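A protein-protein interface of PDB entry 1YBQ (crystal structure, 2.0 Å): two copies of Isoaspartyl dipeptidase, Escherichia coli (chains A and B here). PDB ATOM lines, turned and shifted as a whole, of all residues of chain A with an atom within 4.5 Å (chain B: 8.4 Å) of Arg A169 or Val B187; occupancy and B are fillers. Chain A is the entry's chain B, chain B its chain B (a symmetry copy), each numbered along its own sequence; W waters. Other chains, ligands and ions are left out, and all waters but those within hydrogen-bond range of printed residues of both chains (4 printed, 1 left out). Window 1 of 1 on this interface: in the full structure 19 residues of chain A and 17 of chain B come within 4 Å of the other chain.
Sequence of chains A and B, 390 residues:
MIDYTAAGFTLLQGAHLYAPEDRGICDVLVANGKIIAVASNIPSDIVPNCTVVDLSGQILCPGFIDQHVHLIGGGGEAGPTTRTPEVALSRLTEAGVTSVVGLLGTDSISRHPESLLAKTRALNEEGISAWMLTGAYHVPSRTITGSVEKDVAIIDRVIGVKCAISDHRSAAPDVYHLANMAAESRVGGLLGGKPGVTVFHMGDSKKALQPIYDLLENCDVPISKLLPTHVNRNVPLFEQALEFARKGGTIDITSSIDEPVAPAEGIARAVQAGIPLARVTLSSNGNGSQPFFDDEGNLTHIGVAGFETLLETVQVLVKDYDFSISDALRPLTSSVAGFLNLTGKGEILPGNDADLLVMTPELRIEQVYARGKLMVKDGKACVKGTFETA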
ATOM      1  N   GLU A  77      31.183   4.245  16.098  1.00  0.00           N
ATOM      2  CA  GLU A  77      31.431   3.135  17.043  1.00  0.00           C
ATOM      3  C   GLU A  77      31.614   3.577  18.507  1.00  0.00           C
ATOM      4  O   GLU A  77      31.664   2.776  19.446  1.00  0.00           O
ATOM      5  CB  GLU A  77      32.696   2.344  16.675  1.00  0.00           C
ATOM      6  CG  GLU A  77      32.538   1.493  15.413  1.00  0.00           C
ATOM      7  CD  GLU A  77      32.976   2.141  14.129  1.00  0.00           C
ATOM      8  OE1 GLU A  77      33.044   3.358  13.924  1.00  0.00           O
ATOM      9  OE2 GLU A  77      33.212   1.212  13.244  1.00  0.00           O
ATOM     10  N   THR A 106      29.608   0.173   9.808  1.00  0.00           N
ATOM     11  CA  THR A 106      28.938  -0.213  11.026  1.00  0.00           C
ATOM     12  C   THR A 106      27.553   0.390  11.234  1.00  0.00           C
ATOM     13  O   THR A 106      26.601  -0.270  11.627  1.00  0.00           O
ATOM     14  CB  THR A 106      29.806   0.125  12.253  1.00  0.00           C
ATOM     15  OG1 THR A 106      31.127  -0.346  12.039  1.00  0.00           O
ATOM     16  CG2 THR A 106      29.210  -0.563  13.479  1.00  0.00           C
ATOM     17  N   TYR A 137      26.981  -3.227   7.227  1.00  0.00           N
ATOM     18  CA  TYR A 137      27.437  -4.429   7.912  1.00  0.00           C
ATOM     19  C   TYR A 137      26.285  -5.385   8.171  1.00  0.00           C
ATOM     20  O   TYR A 137      26.421  -6.607   8.084  1.00  0.00           O
ATOM     21  CB  TYR A 137      27.993  -4.070   9.293  1.00  0.00           C
ATOM     22  CG  TYR A 137      29.414  -3.544   9.315  1.00  0.00           C
ATOM     23  CD1 TYR A 137      30.020  -2.980   8.189  1.00  0.00           C
ATOM     24  CD2 TYR A 137      30.133  -3.610  10.507  1.00  0.00           C
ATOM     25  CE1 TYR A 137      31.322  -2.472   8.241  1.00  0.00           C
ATOM     26  CE2 TYR A 137      31.438  -3.126  10.591  1.00  0.00           C
ATOM     27  CZ  TYR A 137      32.017  -2.570   9.451  1.00  0.00           C
ATOM     28  OH  TYR A 137      33.274  -2.091   9.577  1.00  0.00           O
ATOM     29  N   ASP A 167      33.378 -10.556  12.546  1.00  0.00           N
ATOM     30  CA  ASP A 167      33.611  -9.342  13.294  1.00  0.00           C
ATOM     31  C   ASP A 167      32.569  -9.167  14.402  1.00  0.00           C
ATOM     32  O   ASP A 167      31.384  -9.500  14.253  1.00  0.00           O
ATOM     33  CB  ASP A 167      33.531  -8.169  12.305  1.00  0.00           C
ATOM     34  CG  ASP A 167      33.840  -6.830  12.916  1.00  0.00           C
ATOM     35  OD1 ASP A 167      33.107  -6.314  13.735  1.00  0.00           O
ATOM     36  OD2 ASP A 167      34.948  -6.275  12.435  1.00  0.00           O
ATOM     37  N   HIS A 168      33.049  -8.633  15.525  1.00  0.00           N
ATOM     38  CA  HIS A 168      32.213  -8.420  16.705  1.00  0.00           C
ATOM     39  C   HIS A 168      31.136  -7.347  16.494  1.00  0.00           C
ATOM     40  O   HIS A 168      30.394  -6.990  17.411  1.00  0.00           O
ATOM     41  CB  HIS A 168      33.056  -8.104  17.967  1.00  0.00           C
ATOM     42  CG  HIS A 168      33.802  -6.814  17.777  1.00  0.00           C
ATOM     43  ND1 HIS A 168      35.138  -6.794  17.405  1.00  0.00           N
ATOM     44  CD2 HIS A 168      33.358  -5.534  17.856  1.00  0.00           C
ATOM     45  CE1 HIS A 168      35.479  -5.513  17.282  1.00  0.00           C
ATOM     46  NE2 HIS A 168      34.428  -4.731  17.546  1.00  0.00           N
ATOM     47  N   ARG A 169      31.047  -6.807  15.295  1.00  0.00           N
ATOM     48  CA  ARG A 169      30.011  -5.810  15.033  1.00  0.00           C
ATOM     49  C   ARG A 169      29.102  -6.338  13.939  1.00  0.00           C
ATOM     50  O   ARG A 169      28.296  -5.607  13.357  1.00  0.00           O
ATOM     51  CB  ARG A 169      30.627  -4.521  14.543  1.00  0.00           C
ATOM     52  CG  ARG A 169      31.583  -3.929  15.549  1.00  0.00           C
ATOM     53  CD  ARG A 169      32.430  -2.847  14.907  1.00  0.00           C
ATOM     54  NE  ARG A 169      33.484  -3.463  14.113  1.00  0.00           N
ATOM     55  CZ  ARG A 169      34.415  -2.812  13.469  1.00  0.00           C
ATOM     56  NH1 ARG A 169      34.502  -1.470  13.470  1.00  0.00           N
ATOM     57  NH2 ARG A 169      35.274  -3.569  12.797  1.00  0.00           N
ATOM     58  N   SER A 170      29.277  -7.618  13.611  1.00  0.00           N
ATOM     59  CA  SER A 170      28.414  -8.223  12.594  1.00  0.00           C
ATOM     60  C   SER A 170      26.990  -8.377  13.195  1.00  0.00           C
ATOM     61  O   SER A 170      26.775  -8.085  14.369  1.00  0.00           O
ATOM     62  CB  SER A 170      28.958  -9.593  12.184  1.00  0.00           C
ATOM     63  OG  SER A 170      28.606 -10.529  13.204  1.00  0.00           O
ATOM     64  N   ALA A 171      26.013  -8.819  12.392  1.00  0.00           N
ATOM     65  CA  ALA A 171      24.638  -9.013  12.839  1.00  0.00           C
ATOM     66  C   ALA A 171      24.436 -10.505  13.118  1.00  0.00           C
ATOM     67  O   ALA A 171      23.321 -10.983  13.148  1.00  0.00           O
ATOM     68  CB  ALA A 171      23.651  -8.545  11.753  1.00  0.00           C
ATOM     69  N   HIS A 201      33.126  -7.191   4.530  1.00  0.00           N
ATOM     70  CA  HIS A 201      34.108  -6.636   5.418  1.00  0.00           C
ATOM     71  C   HIS A 201      34.512  -7.802   6.326  1.00  0.00           C
ATOM     72  O   HIS A 201      33.652  -8.516   6.851  1.00  0.00           O
ATOM     73  CB  HIS A 201      33.509  -5.470   6.245  1.00  0.00           C
ATOM     74  CG  HIS A 201      34.047  -5.344   7.645  1.00  0.00           C
ATOM     75  ND1 HIS A 201      34.858  -4.266   8.019  1.00  0.00           N
ATOM     76  CD2 HIS A 201      33.901  -6.153   8.743  1.00  0.00           C
ATOM     77  CE1 HIS A 201      35.179  -4.456   9.292  1.00  0.00           C
ATOM     78  NE2 HIS A 201      34.627  -5.579   9.761  1.00  0.00           N
ATOM     79  N   PRO A 291      38.759   2.309  14.178  1.00  0.00           N
ATOM     80  CA  PRO A 291      38.604   1.986  15.575  1.00  0.00           C
ATOM     81  C   PRO A 291      39.413   0.761  15.931  1.00  0.00           C
ATOM     82  O   PRO A 291      39.579  -0.177  15.126  1.00  0.00           O
ATOM     83  CB  PRO A 291      37.110   1.688  15.760  1.00  0.00           C
ATOM     84  CG  PRO A 291      36.609   1.274  14.385  1.00  0.00           C
ATOM     85  CD  PRO A 291      37.647   1.730  13.370  1.00  0.00           C
ATOM     86  N   PHE A 293      39.901  -2.056  19.113  1.00  0.00           N
ATOM     87  CA  PHE A 293      39.215  -2.652  20.236  1.00  0.00           C
ATOM     88  C   PHE A 293      40.181  -3.506  21.024  1.00  0.00           C
ATOM     89  O   PHE A 293      40.961  -4.230  20.415  1.00  0.00           O
ATOM     90  CB  PHE A 293      37.984  -3.485  19.761  1.00  0.00           C
ATOM     91  CG  PHE A 293      36.865  -2.626  19.216  1.00  0.00           C
ATOM     92  CD1 PHE A 293      36.930  -2.058  17.940  1.00  0.00           C
ATOM     93  CD2 PHE A 293      35.738  -2.377  19.996  1.00  0.00           C
ATOM     94  CE1 PHE A 293      35.902  -1.254  17.441  1.00  0.00           C
ATOM     95  CE2 PHE A 293      34.703  -1.571  19.521  1.00  0.00           C
ATOM     96  CZ  PHE A 293      34.786  -1.015  18.242  1.00  0.00           C
ATOM     97  N   VAL B 148      15.742  -4.331  17.700  1.00  0.00           N
ATOM     98  CA  VAL B 148      16.506  -4.332  18.925  1.00  0.00           C
ATOM     99  C   VAL B 148      17.616  -3.317  18.792  1.00  0.00           C
ATOM    100  O   VAL B 148      17.842  -2.437  19.622  1.00  0.00           O
ATOM    101  CB  VAL B 148      17.107  -5.694  19.208  1.00  0.00           C
ATOM    102  CG1 VAL B 148      18.231  -5.564  20.233  1.00  0.00           C
ATOM    103  CG2 VAL B 148      16.021  -6.660  19.684  1.00  0.00           C
ATOM    104  N   GLU B 149      18.305  -3.487  17.679  1.00  0.00           N
ATOM    105  CA  GLU B 149      19.407  -2.628  17.388  1.00  0.00           C
ATOM    106  C   GLU B 149      19.012  -1.150  17.431  1.00  0.00           C
ATOM    107  O   GLU B 149      19.735  -0.310  17.977  1.00  0.00           O
ATOM    108  CB  GLU B 149      20.040  -3.024  16.034  1.00  0.00           C
ATOM    109  CG  GLU B 149      21.302  -2.195  15.680  1.00  0.00           C
ATOM    110  CD  GLU B 149      22.031  -2.635  14.406  1.00  0.00           C
ATOM    111  OE1 GLU B 149      22.089  -1.947  13.393  1.00  0.00           O
ATOM    112  OE2 GLU B 149      22.642  -3.805  14.495  1.00  0.00           O
ATOM    113  N   LYS B 150      17.856  -0.829  16.846  1.00  0.00           N
ATOM    114  CA  LYS B 150      17.430   0.573  16.842  1.00  0.00           C
ATOM    115  C   LYS B 150      17.004   1.029  18.235  1.00  0.00           C
ATOM    116  O   LYS B 150      17.280   2.159  18.659  1.00  0.00           O
ATOM    117  CB  LYS B 150      16.271   0.718  15.862  1.00  0.00           C
ATOM    118  CG  LYS B 150      15.929   2.157  15.498  1.00  0.00           C
ATOM    119  CD  LYS B 150      15.132   2.285  14.199  1.00  0.00           C
ATOM    120  CE  LYS B 150      14.798   3.729  13.815  1.00  0.00           C
ATOM    121  NZ  LYS B 150      13.772   3.884  12.769  1.00  0.00           N
ATOM    122  N   VAL B 152      18.058   0.047  21.128  1.00  0.00           N
ATOM    123  CA  VAL B 152      19.275   0.344  21.889  1.00  0.00           C
ATOM    124  C   VAL B 152      20.038   1.591  21.370  1.00  0.00           C
ATOM    125  O   VAL B 152      20.572   2.409  22.123  1.00  0.00           O
ATOM    126  CB  VAL B 152      20.207  -0.879  21.994  1.00  0.00           C
ATOM    127  CG1 VAL B 152      21.350  -0.563  22.925  1.00  0.00           C
ATOM    128  CG2 VAL B 152      19.490  -2.089  22.578  1.00  0.00           C
ATOM    129  N   ALA B 153      20.135   1.770  20.060  1.00  0.00           N
ATOM    130  CA  ALA B 153      20.865   2.909  19.595  1.00  0.00           C
ATOM    131  C   ALA B 153      20.081   4.185  19.803  1.00  0.00           C
ATOM    132  O   ALA B 153      20.648   5.215  20.119  1.00  0.00           O
ATOM    133  CB  ALA B 153      21.090   2.753  18.099  1.00  0.00           C
ATOM    134  N   ASN B 180      21.495 -13.348  16.494  1.00  0.00           N
ATOM    135  CA  ASN B 180      21.165 -12.109  15.851  1.00  0.00           C
ATOM    136  C   ASN B 180      20.791 -11.021  16.890  1.00  0.00           C
ATOM    137  O   ASN B 180      21.206  -9.849  16.855  1.00  0.00           O
ATOM    138  CB  ASN B 180      20.016 -12.337  14.842  1.00  0.00           C
ATOM    139  CG  ASN B 180      19.506 -10.969  14.327  1.00  0.00           C
ATOM    140  OD1 ASN B 180      20.227 -10.181  13.694  1.00  0.00           O
ATOM    141  ND2 ASN B 180      18.290 -10.606  14.690  1.00  0.00           N
ATOM    142  N   MET B 181      19.976 -11.392  17.854  1.00  0.00           N
ATOM    143  CA  MET B 181      19.511 -10.477  18.892  1.00  0.00           C
ATOM    144  C   MET B 181      20.640  -9.868  19.732  1.00  0.00           C
ATOM    145  O   MET B 181      20.721  -8.669  19.973  1.00  0.00           O
ATOM    146  CB  MET B 181      18.484 -11.233  19.777  1.00  0.00           C
ATOM    147  CG  MET B 181      17.914 -10.434  20.944  1.00  0.00           C
ATOM    148  SD  MET B 181      17.164 -11.468  22.237  1.00  0.00           S
ATOM    149  CE  MET B 181      18.656 -12.331  22.792  1.00  0.00           C
ATOM    150  N   ALA B 182      21.534 -10.728  20.187  1.00  0.00           N
ATOM    151  CA  ALA B 182      22.657 -10.274  20.964  1.00  0.00           C
ATOM    152  C   ALA B 182      23.569  -9.344  20.126  1.00  0.00           C
ATOM    153  O   ALA B 182      24.115  -8.338  20.619  1.00  0.00           O
ATOM    154  CB  ALA B 182      23.423 -11.495  21.458  1.00  0.00           C
ATOM    155  N   ALA B 183      23.737  -9.701  18.841  1.00  0.00           N
ATOM    156  CA  ALA B 183      24.565  -8.922  17.948  1.00  0.00           C
ATOM    157  C   ALA B 183      23.929  -7.531  17.733  1.00  0.00           C
ATOM    158  O   ALA B 183      24.625  -6.517  17.660  1.00  0.00           O
ATOM    159  CB  ALA B 183      24.765  -9.676  16.650  1.00  0.00           C
ATOM    160  N   GLU B 184      22.598  -7.482  17.690  1.00  0.00           N
ATOM    161  CA  GLU B 184      21.930  -6.202  17.494  1.00  0.00           C
ATOM    162  C   GLU B 184      22.063  -5.280  18.679  1.00  0.00           C
ATOM    163  O   GLU B 184      22.160  -4.062  18.560  1.00  0.00           O
ATOM    164  CB  GLU B 184      20.447  -6.415  17.218  1.00  0.00           C
ATOM    165  CG  GLU B 184      20.245  -6.883  15.789  1.00  0.00           C
ATOM    166  CD  GLU B 184      18.943  -6.434  15.188  1.00  0.00           C
ATOM    167  OE1 GLU B 184      18.103  -5.792  15.800  1.00  0.00           O
ATOM    168  OE2 GLU B 184      18.824  -6.813  13.939  1.00  0.00           O
ATOM    169  N   SER B 185      22.007  -5.880  19.856  1.00  0.00           N
ATOM    170  CA  SER B 185      22.142  -5.124  21.105  1.00  0.00           C
ATOM    171  C   SER B 185      23.572  -4.608  21.191  1.00  0.00           C
ATOM    172  O   SER B 185      23.824  -3.432  21.475  1.00  0.00           O
ATOM    173  CB  SER B 185      21.772  -5.971  22.329  1.00  0.00           C
ATOM    174  OG  SER B 185      21.785  -5.213  23.517  1.00  0.00           O
ATOM    175  N   ARG B 186      24.534  -5.494  20.908  1.00  0.00           N
ATOM    176  CA  ARG B 186      25.931  -5.084  20.928  1.00  0.00           C
ATOM    177  C   ARG B 186      26.182  -3.855  20.028  1.00  0.00           C
ATOM    178  O   ARG B 186      26.639  -2.806  20.441  1.00  0.00           O
ATOM    179  CB  ARG B 186      26.806  -6.268  20.561  1.00  0.00           C
ATOM    180  CG  ARG B 186      28.249  -6.005  20.906  1.00  0.00           C
ATOM    181  CD  ARG B 186      28.913  -5.159  19.827  1.00  0.00           C
ATOM    182  NE  ARG B 186      30.359  -5.370  19.776  1.00  0.00           N
ATOM    183  CZ  ARG B 186      31.234  -4.820  20.610  1.00  0.00           C
ATOM    184  NH1 ARG B 186      30.829  -4.008  21.565  1.00  0.00           N
ATOM    185  NH2 ARG B 186      32.543  -5.066  20.486  1.00  0.00           N
ATOM    186  N   VAL B 187      25.799  -3.963  18.767  1.00  0.00           N
ATOM    187  CA  VAL B 187      25.930  -2.874  17.819  1.00  0.00           C
ATOM    188  C   VAL B 187      25.119  -1.609  18.198  1.00  0.00           C
ATOM    189  O   VAL B 187      25.671  -0.508  18.205  1.00  0.00           O
ATOM    190  CB  VAL B 187      25.674  -3.363  16.405  1.00  0.00           C
ATOM    191  CG1 VAL B 187      25.741  -2.157  15.474  1.00  0.00           C
ATOM    192  CG2 VAL B 187      26.713  -4.448  16.054  1.00  0.00           C
ATOM    193  N   GLY B 188      23.843  -1.739  18.568  1.00  0.00           N
ATOM    194  CA  GLY B 188      23.062  -0.574  18.965  1.00  0.00           C
ATOM    195  C   GLY B 188      23.750   0.170  20.120  1.00  0.00           C
ATOM    196  O   GLY B 188      23.766   1.394  20.212  1.00  0.00           O
ATOM    197  N   GLY B 189      24.359  -0.633  20.979  1.00  0.00           N
ATOM    198  CA  GLY B 189      25.087  -0.172  22.137  1.00  0.00           C
ATOM    199  C   GLY B 189      26.242   0.726  21.740  1.00  0.00           C
ATOM    200  O   GLY B 189      26.400   1.799  22.314  1.00  0.00           O
ATOM    201  N   LEU B 190      27.055   0.260  20.787  1.00  0.00           N
ATOM    202  CA  LEU B 190      28.156   1.071  20.349  1.00  0.00           C
ATOM    203  C   LEU B 190      27.611   2.341  19.748  1.00  0.00           C
ATOM    204  O   LEU B 190      28.126   3.416  19.917  1.00  0.00           O
ATOM    205  CB  LEU B 190      29.001   0.382  19.281  1.00  0.00           C
ATOM    206  CG  LEU B 190      29.583  -0.952  19.777  1.00  0.00           C
ATOM    207  CD1 LEU B 190      30.362  -1.591  18.631  1.00  0.00           C
ATOM    208  CD2 LEU B 190      30.590  -0.670  20.859  1.00  0.00           C
ATOM    209  N   LEU B 191      26.558   2.244  19.000  1.00  0.00           N
ATOM    210  CA  LEU B 191      26.068   3.454  18.376  1.00  0.00           C
ATOM    211  C   LEU B 191      25.459   4.431  19.345  1.00  0.00           C
ATOM    212  O   LEU B 191      25.559   5.657  19.183  1.00  0.00           O
ATOM    213  CB  LEU B 191      25.003   3.163  17.292  1.00  0.00           C
ATOM    214  CG  LEU B 191      25.472   2.267  16.138  1.00  0.00           C
ATOM    215  CD1 LEU B 191      24.332   2.083  15.130  1.00  0.00           C
ATOM    216  CD2 LEU B 191      26.712   2.817  15.424  1.00  0.00           C
ATOM    217  N   GLY B 192      24.751   3.915  20.324  1.00  0.00           N
ATOM    218  CA  GLY B 192      24.105   4.874  21.217  1.00  0.00           C
ATOM    219  C   GLY B 192      24.880   5.198  22.494  1.00  0.00           C
ATOM    220  O   GLY B 192      24.451   6.007  23.310  1.00  0.00           O
ATOM    221  N   GLY B 193      26.029   4.555  22.698  1.00  0.00           N
ATOM    222  CA  GLY B 193      26.778   4.797  23.899  1.00  0.00           C
ATOM    223  C   GLY B 193      26.231   3.959  25.048  1.00  0.00           C
ATOM    224  O   GLY B 193      26.210   4.393  26.202  1.00  0.00           O
ATOM    225  N   LYS B 194      25.750   2.762  24.751  1.00  0.00           N
ATOM    226  CA  LYS B 194      25.190   1.941  25.826  1.00  0.00           C
ATOM    227  C   LYS B 194      26.080   0.728  25.968  1.00  0.00           C
ATOM    228  O   LYS B 194      26.875   0.424  25.094  1.00  0.00           O
ATOM    229  CB  LYS B 194      23.768   1.470  25.493  1.00  0.00           C
ATOM    230  CG  LYS B 194      22.913   2.499  24.732  1.00  0.00           C
ATOM    231  CD  LYS B 194      22.456   3.652  25.606  1.00  0.00           C
ATOM    232  CE  LYS B 194      21.529   4.641  24.880  1.00  0.00           C
ATOM    233  NZ  LYS B 194      20.321   4.038  24.350  1.00  0.00           N
ATOM    234  N   PRO B 195      25.946   0.040  27.061  1.00  0.00           N
ATOM    235  CA  PRO B 195      26.733  -1.162  27.249  1.00  0.00           C
ATOM    236  C   PRO B 195      26.340  -2.207  26.211  1.00  0.00           C
ATOM    237  O   PRO B 195      27.175  -3.007  25.808  1.00  0.00           O
ATOM    238  CB  PRO B 195      26.453  -1.667  28.665  1.00  0.00           C
ATOM    239  CG  PRO B 195      25.299  -0.812  29.176  1.00  0.00           C
ATOM    240  CD  PRO B 195      25.282   0.442  28.326  1.00  0.00           C
ATOM    241  N   GLY B 196      25.063  -2.199  25.772  1.00  0.00           N
ATOM    242  CA  GLY B 196      24.547  -3.131  24.748  1.00  0.00           C
ATOM    243  C   GLY B 196      24.608  -4.610  25.155  1.00  0.00           C
ATOM    244  O   GLY B 196      25.095  -5.500  24.446  1.00  0.00           O
ATOM    245  N   VAL B 197      24.088  -4.860  26.344  1.00  0.00           N
ATOM    246  CA  VAL B 197      24.109  -6.188  26.865  1.00  0.00           C
ATOM    247  C   VAL B 197      22.861  -6.964  26.543  1.00  0.00           C
ATOM    248  O   VAL B 197      21.805  -6.410  26.191  1.00  0.00           O
ATOM    249  CB  VAL B 197      24.284  -6.088  28.365  1.00  0.00           C
ATOM    250  CG1 VAL B 197      25.673  -5.529  28.664  1.00  0.00           C
ATOM    251  CG2 VAL B 197      23.208  -5.154  28.964  1.00  0.00           C
ATOM    252  N   CYS B 219      28.646 -16.574  16.650  1.00  0.00           N
ATOM    253  CA  CYS B 219      28.759 -15.156  16.510  1.00  0.00           C
ATOM    254  C   CYS B 219      29.995 -14.639  17.198  1.00  0.00           C
ATOM    255  O   CYS B 219      30.744 -15.396  17.792  1.00  0.00           O
ATOM    256  CB  CYS B 219      27.465 -14.400  16.829  1.00  0.00           C
ATOM    257  SG  CYS B 219      27.333 -14.270  18.608  1.00  0.00           S
ATOM    258  N   ASP B 220      30.203 -13.347  17.079  1.00  0.00           N
ATOM    259  CA  ASP B 220      31.393 -12.757  17.649  1.00  0.00           C
ATOM    260  C   ASP B 220      31.136 -11.744  18.730  1.00  0.00           C
ATOM    261  O   ASP B 220      32.003 -10.891  18.970  1.00  0.00           O
ATOM    262  CB  ASP B 220      32.297 -12.196  16.546  1.00  0.00           C
ATOM    263  CG  ASP B 220      32.815 -13.318  15.698  1.00  0.00           C
ATOM    264  OD1 ASP B 220      33.555 -14.188  16.148  1.00  0.00           O
ATOM    265  OD2 ASP B 220      32.364 -13.266  14.461  1.00  0.00           O
ATOM    266  N   VAL B 221      29.962 -11.842  19.384  1.00  0.00           N
ATOM    267  CA  VAL B 221      29.662 -10.925  20.492  1.00  0.00           C
ATOM    268  C   VAL B 221      30.585 -11.268  21.684  1.00  0.00           C
ATOM    269  O   VAL B 221      30.728 -12.450  22.037  1.00  0.00           O
ATOM    270  CB  VAL B 221      28.176 -10.924  20.901  1.00  0.00           C
ATOM    271  CG1 VAL B 221      27.906  -9.824  21.925  1.00  0.00           C
ATOM    272  CG2 VAL B 221      27.266 -10.706  19.695  1.00  0.00           C
ATOM    273  N   PRO B 222      31.221 -10.256  22.295  1.00  0.00           N
ATOM    274  CA  PRO B 222      32.106 -10.515  23.428  1.00  0.00           C
ATOM    275  C   PRO B 222      31.358 -11.093  24.623  1.00  0.00           C
ATOM    276  O   PRO B 222      30.264 -10.647  24.973  1.00  0.00           O
ATOM    277  CB  PRO B 222      32.684  -9.159  23.820  1.00  0.00           C
ATOM    278  CG  PRO B 222      32.328  -8.166  22.715  1.00  0.00           C
ATOM    279  CD  PRO B 222      31.233  -8.815  21.897  1.00  0.00           C
ATOM    280  N   LYS B 225      29.295  -9.224  27.224  1.00  0.00           N
ATOM    281  CA  LYS B 225      28.020  -8.525  27.002  1.00  0.00           C
ATOM    282  C   LYS B 225      26.852  -9.425  27.401  1.00  0.00           C
ATOM    283  O   LYS B 225      25.683  -9.020  27.376  1.00  0.00           O
ATOM    284  CB  LYS B 225      27.840  -8.160  25.537  1.00  0.00           C
ATOM    285  CG  LYS B 225      28.870  -7.174  25.077  1.00  0.00           C
ATOM    286  CD  LYS B 225      28.817  -5.853  25.835  1.00  0.00           C
ATOM    287  CE  LYS B 225      29.963  -4.913  25.445  1.00  0.00           C
ATOM    288  NZ  LYS B 225      29.972  -3.583  26.091  1.00  0.00           N
HETATM  289  O   HOH W   1      24.443  -2.997  11.924  1.00  0.00           O
HETATM  290  O   HOH W   2      30.172 -12.533  13.262  1.00  0.00           O
HETATM  291  O   HOH W   3      23.799  -0.072  12.257  1.00  0.00           O
HETATM  292  O   HOH W   4      28.722 -11.190  16.044  1.00  0.00           O
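Glu A77 touches Leu B190 (O to CB, 3.6 Å). CB of His A168 touches O of Asp B220, 3.1 Å away. Arg A169 touches Val B187 (O to CG2, 3.3 Å). Ala B183 touches Ser A170 (CB to O, 3.4 Å). Ala B183 touches Ala A171 (CB to C, 3.6 Å).
Printed residues of chain B within 4 Å of Glu A77: Leu B190 (3.6 Å). Of the printed residues of chain B, Asp A167 touches Asp B220 (3.5 Å). Printed residues of chain B within 4 Å of Arg A169: Val B187 (3.3 Å). Printed residues of chain A within 4 Å of Asn B180: Ala A171. Ala B182 touches none of the printed residues of chain A. Of the printed residues of chain A, Arg B186 touches His A168 (2.8 Å). Of the printed residues of chain A, Val B187 touches Arg A169 (3.3 Å). Gly B188 touches none of the printed residues of chain A. Printed residues of chain A within 4 Å of Leu B190: Glu A77. The nearest residue of chain B that does not touch Arg A169 is Leu B190 (4.1 Å). The nearest printed residue of chain A that does not touch Val B187 is Ser A170 (4.01 Å). The nearest printed residue of chain B that does not touch Glu A77 is Leu B191 (4.7 Å).
The side-chain carboxylate (OD2) of Asp B220 sits at hydrogen-bond distance from the backbone NH (N) of Asp A167 (3.5 Å). The backbone carbonyl oxygen (O) of His A168 lies within hydrogen-bond range of the guanidinium group (NE) of Arg B186 (2.9 Å). O of Ala A171 lies close to OD1 of Asn B180 (3.2 Å).
Water W2 lies within hydrogen-bond range of OG of Ser A170 (2.5 Å), OD2 of Asp B220 (2.6 Å) and O of Asp A167 (3.4 Å). Water W3 lies within hydrogen-bond range of the side-chain carboxylate of Glu B149 and the backbone carbonyl oxygen of Thr A106. Water W4 lies within hydrogen-bond range of N of Asp B220 (2.8 Å) and OG of Ser A170 (2.9 Å). Water W1 bridges the side-chain carboxylate (OE1) of Glu B149 and the backbone carbonyl oxygen (O) of Thr A106.
Of the 28 printed residues of chain B, 6 touch a printed residue of chain A. Hydrophobic or aromatic side chains of chain B within 4 Å of the printed part of chain A: Ala B183, Val B187 and Leu B190. Of the 11 printed residues of chain A, 6 touch a printed residue of chain B. Hydrophobic or aromatic side chains of chain A that line the printed part of chain B: His A168. Along chain A the printed residues that touch a printed residue of chain B span positions 77 to 171. Among the printed residues, 8 pairs touch across the chains.
The side-chain carboxylate (OD2) of Asp A167 is in hydrogen-bond range of a ring nitrogen (NE2) of His A201 (2.8 Å). The guanidinium group (NH2) of Arg A169 is in salt-bridge range of the side-chain carboxylate (OD2) of Asp A167. OE2 of Glu A77 sits at hydrogen-bond distance from OG1 of Thr A106 (2.9 Å). O of Asp A167 is in hydrogen-bond range of OG of Ser A170 (3.1 Å). OE2 of Glu A77 lies within salt-bridge range of NH1 of Arg A169 (3.0 Å).
No position is printed for both chains.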
